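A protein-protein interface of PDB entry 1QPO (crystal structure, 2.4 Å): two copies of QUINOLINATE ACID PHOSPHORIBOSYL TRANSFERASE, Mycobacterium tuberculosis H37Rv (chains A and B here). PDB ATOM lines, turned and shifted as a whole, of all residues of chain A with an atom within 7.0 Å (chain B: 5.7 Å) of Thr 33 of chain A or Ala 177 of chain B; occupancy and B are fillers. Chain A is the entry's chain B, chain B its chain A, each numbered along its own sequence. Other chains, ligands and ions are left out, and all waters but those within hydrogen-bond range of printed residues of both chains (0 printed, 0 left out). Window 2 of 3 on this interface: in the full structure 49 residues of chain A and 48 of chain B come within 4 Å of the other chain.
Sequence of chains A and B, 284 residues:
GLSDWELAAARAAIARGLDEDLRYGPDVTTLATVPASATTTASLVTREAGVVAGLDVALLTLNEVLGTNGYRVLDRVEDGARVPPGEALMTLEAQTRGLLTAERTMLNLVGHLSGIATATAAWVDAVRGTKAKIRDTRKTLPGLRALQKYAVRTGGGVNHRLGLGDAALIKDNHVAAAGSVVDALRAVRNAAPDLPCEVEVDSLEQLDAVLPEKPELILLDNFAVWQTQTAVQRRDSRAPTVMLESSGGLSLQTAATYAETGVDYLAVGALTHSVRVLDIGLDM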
ATOM      1  N   ASP A  27      14.764  15.693  29.943  1.00  0.00           N
ATOM      2  CA  ASP A  27      16.086  15.843  29.401  1.00  0.00           C
ATOM      3  C   ASP A  27      15.952  16.150  27.921  1.00  0.00           C
ATOM      4  O   ASP A  27      16.034  15.274  27.060  1.00  0.00           O
ATOM      5  CB  ASP A  27      16.876  14.565  29.642  1.00  0.00           C
ATOM      6  CG  ASP A  27      18.363  14.748  29.419  1.00  0.00           C
ATOM      7  OD1 ASP A  27      18.777  15.781  28.825  1.00  0.00           O
ATOM      8  OD2 ASP A  27      19.121  13.837  29.842  1.00  0.00           O
ATOM      9  N   VAL A  28      15.746  17.416  27.637  1.00  0.00           N
ATOM     10  CA  VAL A  28      15.572  17.868  26.276  1.00  0.00           C
ATOM     11  C   VAL A  28      16.619  17.371  25.295  1.00  0.00           C
ATOM     12  O   VAL A  28      16.312  17.088  24.143  1.00  0.00           O
ATOM     13  CB  VAL A  28      15.502  19.414  26.217  1.00  0.00           C
ATOM     14  CG1 VAL A  28      16.631  20.033  27.037  1.00  0.00           C
ATOM     15  CG2 VAL A  28      15.573  19.899  24.793  1.00  0.00           C
ATOM     16  N   THR A  29      17.853  17.230  25.750  1.00  0.00           N
ATOM     17  CA  THR A  29      18.901  16.796  24.841  1.00  0.00           C
ATOM     18  C   THR A  29      18.849  15.313  24.437  1.00  0.00           C
ATOM     19  O   THR A  29      19.192  14.971  23.303  1.00  0.00           O
ATOM     20  CB  THR A  29      20.321  17.297  25.301  1.00  0.00           C
ATOM     21  OG1 THR A  29      21.355  16.578  24.601  1.00  0.00           O
ATOM     22  CG2 THR A  29      20.491  17.193  26.831  1.00  0.00           C
ATOM     23  N   THR A  30      18.415  14.425  25.329  1.00  0.00           N
ATOM     24  CA  THR A  30      18.318  13.026  24.922  1.00  0.00           C
ATOM     25  C   THR A  30      17.056  12.862  24.098  1.00  0.00           C
ATOM     26  O   THR A  30      16.994  11.995  23.259  1.00  0.00           O
ATOM     27  CB  THR A  30      18.328  12.002  26.083  1.00  0.00           C
ATOM     28  OG1 THR A  30      17.000  11.562  26.401  1.00  0.00           O
ATOM     29  CG2 THR A  30      18.945  12.584  27.261  1.00  0.00           C
ATOM     30  N   LEU A  31      16.051  13.688  24.367  1.00  0.00           N
ATOM     31  CA  LEU A  31      14.810  13.656  23.599  1.00  0.00           C
ATOM     32  C   LEU A  31      15.141  14.033  22.155  1.00  0.00           C
ATOM     33  O   LEU A  31      14.700  13.379  21.216  1.00  0.00           O
ATOM     34  CB  LEU A  31      13.806  14.647  24.170  1.00  0.00           C
ATOM     35  CG  LEU A  31      12.825  14.029  25.150  1.00  0.00           C
ATOM     36  CD1 LEU A  31      13.575  13.250  26.199  1.00  0.00           C
ATOM     37  CD2 LEU A  31      11.984  15.119  25.785  1.00  0.00           C
ATOM     38  N   ALA A  32      15.965  15.065  21.993  1.00  0.00           N
ATOM     39  CA  ALA A  32      16.374  15.540  20.682  1.00  0.00           C
ATOM     40  C   ALA A  32      17.381  14.658  19.960  1.00  0.00           C
ATOM     41  O   ALA A  32      17.354  14.602  18.735  1.00  0.00           O
ATOM     42  CB  ALA A  32      16.915  16.932  20.794  1.00  0.00           C
ATOM     43  N   THR A  33      18.253  13.960  20.686  1.00  0.00           N
ATOM     44  CA  THR A  33      19.271  13.126  20.032  1.00  0.00           C
ATOM     45  C   THR A  33      19.022  11.618  19.934  1.00  0.00           C
ATOM     46  O   THR A  33      19.464  10.969  18.972  1.00  0.00           O
ATOM     47  CB  THR A  33      20.665  13.371  20.634  1.00  0.00           C
ATOM     48  OG1 THR A  33      20.643  13.123  22.052  1.00  0.00           O
ATOM     49  CG2 THR A  33      21.079  14.807  20.387  1.00  0.00           C
ATOM     50  N   VAL A  34      18.309  11.062  20.912  1.00  0.00           N
ATOM     51  CA  VAL A  34      18.031   9.625  20.941  1.00  0.00           C
ATOM     52  C   VAL A  34      16.551   9.225  20.862  1.00  0.00           C
ATOM     53  O   VAL A  34      15.682   9.695  21.609  1.00  0.00           O
ATOM     54  CB  VAL A  34      18.792   8.878  22.133  1.00  0.00           C
ATOM     55  CG1 VAL A  34      19.457   9.875  23.103  1.00  0.00           C
ATOM     56  CG2 VAL A  34      17.883   7.912  22.877  1.00  0.00           C
ATOM     57  N   PRO A  35      16.238   8.386  19.885  1.00  0.00           N
ATOM     58  CA  PRO A  35      14.886   7.901  19.666  1.00  0.00           C
ATOM     59  C   PRO A  35      14.363   7.027  20.815  1.00  0.00           C
ATOM     60  O   PRO A  35      15.115   6.310  21.478  1.00  0.00           O
ATOM     61  CB  PRO A  35      15.029   7.122  18.357  1.00  0.00           C
ATOM     62  CG  PRO A  35      16.460   6.721  18.329  1.00  0.00           C
ATOM     63  CD  PRO A  35      17.134   7.943  18.810  1.00  0.00           C
ATOM     64  N   THR A  96      17.412   3.339  26.083  1.00  0.00           N
ATOM     65  CA  THR A  96      18.404   4.370  26.248  1.00  0.00           C
ATOM     66  C   THR A  96      17.967   5.646  26.927  1.00  0.00           C
ATOM     67  O   THR A  96      18.653   6.135  27.812  1.00  0.00           O
ATOM     68  CB  THR A  96      19.075   4.636  24.935  1.00  0.00           C
ATOM     69  OG1 THR A  96      19.473   3.364  24.392  1.00  0.00           O
ATOM     70  CG2 THR A  96      20.301   5.533  25.130  1.00  0.00           C
ATOM     71  N   ARG A  97      16.817   6.180  26.567  1.00  0.00           N
ATOM     72  CA  ARG A  97      16.346   7.400  27.212  1.00  0.00           C
ATOM     73  C   ARG A  97      16.172   7.181  28.711  1.00  0.00           C
ATOM     74  O   ARG A  97      16.512   8.055  29.535  1.00  0.00           O
ATOM     75  CB  ARG A  97      15.014   7.856  26.605  1.00  0.00           C
ATOM     76  CG  ARG A  97      15.108   8.404  25.214  1.00  0.00           C
ATOM     77  CD  ARG A  97      13.739   8.828  24.717  1.00  0.00           C
ATOM     78  NE  ARG A  97      13.848   9.539  23.448  1.00  0.00           N
ATOM     79  CZ  ARG A  97      12.826  10.097  22.819  1.00  0.00           C
ATOM     80  NH1 ARG A  97      11.602  10.034  23.341  1.00  0.00           N
ATOM     81  NH2 ARG A  97      13.031  10.685  21.650  1.00  0.00           N
ATOM     82  N   LEU A 100      19.594   7.185  30.508  1.00  0.00           N
ATOM     83  CA  LEU A 100      20.126   8.544  30.657  1.00  0.00           C
ATOM     84  C   LEU A 100      19.369   9.399  31.694  1.00  0.00           C
ATOM     85  O   LEU A 100      19.935  10.285  32.326  1.00  0.00           O
ATOM     86  CB  LEU A 100      20.173   9.239  29.302  1.00  0.00           C
ATOM     87  CG  LEU A 100      21.451   9.036  28.475  1.00  0.00           C
ATOM     88  CD1 LEU A 100      22.144   7.743  28.815  1.00  0.00           C
ATOM     89  CD2 LEU A 100      21.156   9.083  27.008  1.00  0.00           C
ATOM     90  N   ASP B 172      28.836  12.634  25.572  1.00  0.00           N
ATOM     91  CA  ASP B 172      29.249  11.525  24.701  1.00  0.00           C
ATOM     92  C   ASP B 172      28.090  10.705  24.133  1.00  0.00           C
ATOM     93  O   ASP B 172      28.065  10.408  22.942  1.00  0.00           O
ATOM     94  CB  ASP B 172      30.186  10.598  25.496  1.00  0.00           C
ATOM     95  CG  ASP B 172      29.724  10.392  26.960  1.00  0.00           C
ATOM     96  OD1 ASP B 172      29.935  11.297  27.820  1.00  0.00           O
ATOM     97  OD2 ASP B 172      29.137   9.321  27.247  1.00  0.00           O
ATOM     98  N   ASN B 173      27.144  10.346  25.003  1.00  0.00           N
ATOM     99  CA  ASN B 173      25.960   9.561  24.648  1.00  0.00           C
ATOM    100  C   ASN B 173      25.135  10.249  23.570  1.00  0.00           C
ATOM    101  O   ASN B 173      24.696   9.619  22.615  1.00  0.00           O
ATOM    102  CB  ASN B 173      25.081   9.347  25.878  1.00  0.00           C
ATOM    103  CG  ASN B 173      25.859   8.813  27.071  1.00  0.00           C
ATOM    104  OD1 ASN B 173      26.391   7.704  27.039  1.00  0.00           O
ATOM    105  ND2 ASN B 173      25.938   9.607  28.129  1.00  0.00           N
ATOM    106  N   HIS B 174      24.917  11.547  23.735  1.00  0.00           N
ATOM    107  CA  HIS B 174      24.145  12.325  22.771  1.00  0.00           C
ATOM    108  C   HIS B 174      24.941  12.465  21.473  1.00  0.00           C
ATOM    109  O   HIS B 174      24.386  12.369  20.368  1.00  0.00           O
ATOM    110  CB  HIS B 174      23.857  13.705  23.347  1.00  0.00           C
ATOM    111  CG  HIS B 174      23.258  13.666  24.712  1.00  0.00           C
ATOM    112  ND1 HIS B 174      22.113  12.956  24.998  1.00  0.00           N
ATOM    113  CD2 HIS B 174      23.660  14.222  25.878  1.00  0.00           C
ATOM    114  CE1 HIS B 174      21.837  13.080  26.284  1.00  0.00           C
ATOM    115  NE2 HIS B 174      22.758  13.844  26.841  1.00  0.00           N
ATOM    116  N   VAL B 175      26.240  12.711  21.640  1.00  0.00           N
ATOM    117  CA  VAL B 175      27.196  12.854  20.544  1.00  0.00           C
ATOM    118  C   VAL B 175      27.147  11.613  19.634  1.00  0.00           C
ATOM    119  O   VAL B 175      27.094  11.726  18.405  1.00  0.00           O
ATOM    120  CB  VAL B 175      28.632  12.975  21.112  1.00  0.00           C
ATOM    121  CG1 VAL B 175      29.651  12.936  20.002  1.00  0.00           C
ATOM    122  CG2 VAL B 175      28.772  14.229  21.935  1.00  0.00           C
ATOM    123  N   ALA B 176      27.187  10.435  20.262  1.00  0.00           N
ATOM    124  CA  ALA B 176      27.153   9.152  19.562  1.00  0.00           C
ATOM    125  C   ALA B 176      25.881   9.009  18.726  1.00  0.00           C
ATOM    126  O   ALA B 176      25.942   8.806  17.513  1.00  0.00           O
ATOM    127  CB  ALA B 176      27.256   7.995  20.580  1.00  0.00           C
ATOM    128  N   ALA B 177      24.737   9.133  19.393  1.00  0.00           N
ATOM    129  CA  ALA B 177      23.435   9.018  18.760  1.00  0.00           C
ATOM    130  C   ALA B 177      23.301  10.016  17.624  1.00  0.00           C
ATOM    131  O   ALA B 177      22.706   9.713  16.591  1.00  0.00           O
ATOM    132  CB  ALA B 177      22.332   9.242  19.793  1.00  0.00           C
ATOM    133  N   ALA B 178      23.834  11.216  17.824  1.00  0.00           N
ATOM    134  CA  ALA B 178      23.772  12.256  16.803  1.00  0.00           C
ATOM    135  C   ALA B 178      24.749  11.944  15.687  1.00  0.00           C
ATOM    136  O   ALA B 178      24.562  12.356  14.540  1.00  0.00           O
ATOM    137  CB  ALA B 178      24.118  13.587  17.406  1.00  0.00           C
ATOM    138  N   GLY B 179      25.801  11.222  16.049  1.00  0.00           N
ATOM    139  CA  GLY B 179      26.842  10.875  15.109  1.00  0.00           C
ATOM    140  C   GLY B 179      28.076  11.520  15.688  1.00  0.00           C
ATOM    141  O   GLY B 179      29.023  10.830  16.076  1.00  0.00           O
ATOM    142  N   ALA B 184      25.055  16.509  17.401  1.00  0.00           N
ATOM    143  CA  ALA B 184      24.218  16.619  18.597  1.00  0.00           C
ATOM    144  C   ALA B 184      23.918  18.080  18.922  1.00  0.00           C
ATOM    145  O   ALA B 184      22.771  18.470  19.118  1.00  0.00           O
ATOM    146  CB  ALA B 184      24.914  15.962  19.772  1.00  0.00           C
ATOM    147  N   ALA B 187      21.346  19.374  16.632  1.00  0.00           N
ATOM    148  CA  ALA B 187      20.049  18.750  16.904  1.00  0.00           C
ATOM    149  C   ALA B 187      19.318  19.430  18.055  1.00  0.00           C
ATOM    150  O   ALA B 187      18.168  19.843  17.925  1.00  0.00           O
ATOM    151  CB  ALA B 187      20.231  17.274  17.214  1.00  0.00           C
ATOM    152  N   VAL B 188      19.999  19.550  19.181  1.00  0.00           N
ATOM    153  CA  VAL B 188      19.408  20.163  20.353  1.00  0.00           C
ATOM    154  C   VAL B 188      19.090  21.625  20.120  1.00  0.00           C
ATOM    155  O   VAL B 188      18.071  22.115  20.603  1.00  0.00           O
ATOM    156  CB  VAL B 188      20.330  20.013  21.564  1.00  0.00           C
ATOM    157  CG1 VAL B 188      19.768  20.760  22.777  1.00  0.00           C
ATOM    158  CG2 VAL B 188      20.520  18.534  21.855  1.00  0.00           C
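A ring nitrogen (ND1) of His 174 of chain B sits at hydrogen-bond distance from the side-chain hydroxyl (OG1) of Thr 33 of chain A.
The side-chain hydroxyl (OG1) of Thr 33 of chain A is in hydrogen-bond range of the backbone carbonyl oxygen (O) of Thr 29 of chain A.
Among the printed residues, merely in contact across the chains: Thr 30 of chain A with His 174 of chain B (3.1 Å), Thr 33 of chain A with Ala 177 of chain B (3.4 Å), Thr 29 of chain A with Val 188 of chain B (3.5 Å) and Thr 29 of chain A with His 174 of chain B (3.5 Å).
Thr 33 of chain A touches just these residues of chain B: His 174 and Ala 177. Of chain A, only Thr 33 (3.4 Å) comes within 4 Å of Ala 177 of chain B. Of the printed residues of chain B, Thr 30 of chain A touches His 174. Printed residues of chain A within 4 Å of Val 188 of chain B: Thr 29. Printed residues of chain A within 4 Å of His 174 of chain B: Thr 29, Thr 30 and Thr 33. Printed residues of chain B within 4 Å of Thr 29 of chain A: His 174 and Val 188. Ala 187 of chain B touches none of the printed residues of chain A. Ala 176 of chain B touches none of the printed residues of chain A. The nearest printed residue of chain B that does not touch Thr 33 of chain A is Ala 184 of chain B (4.04 Å). The nearest residue of chain A that does not touch Ala 177 of chain B is Val 34 of chain A (4.3 Å). The nearest printed residue of chain A that does not touch Val 188 of chain B is Thr 33 of chain A (4.04 Å).
Along chain B the printed residues that touch a printed residue of chain A span positions 174 to 188. Among the printed residues, 5 pairs touch across the chains. Among the printed residues, no Asp or Glu carboxylate lies within 4 Å of a Lys or Arg side-chain nitrogen of the other chain.
No position is printed for both chains. Of the 5 pairs that touch across the chains among the printed residues, none has its exchanged pair printed and touching as well.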
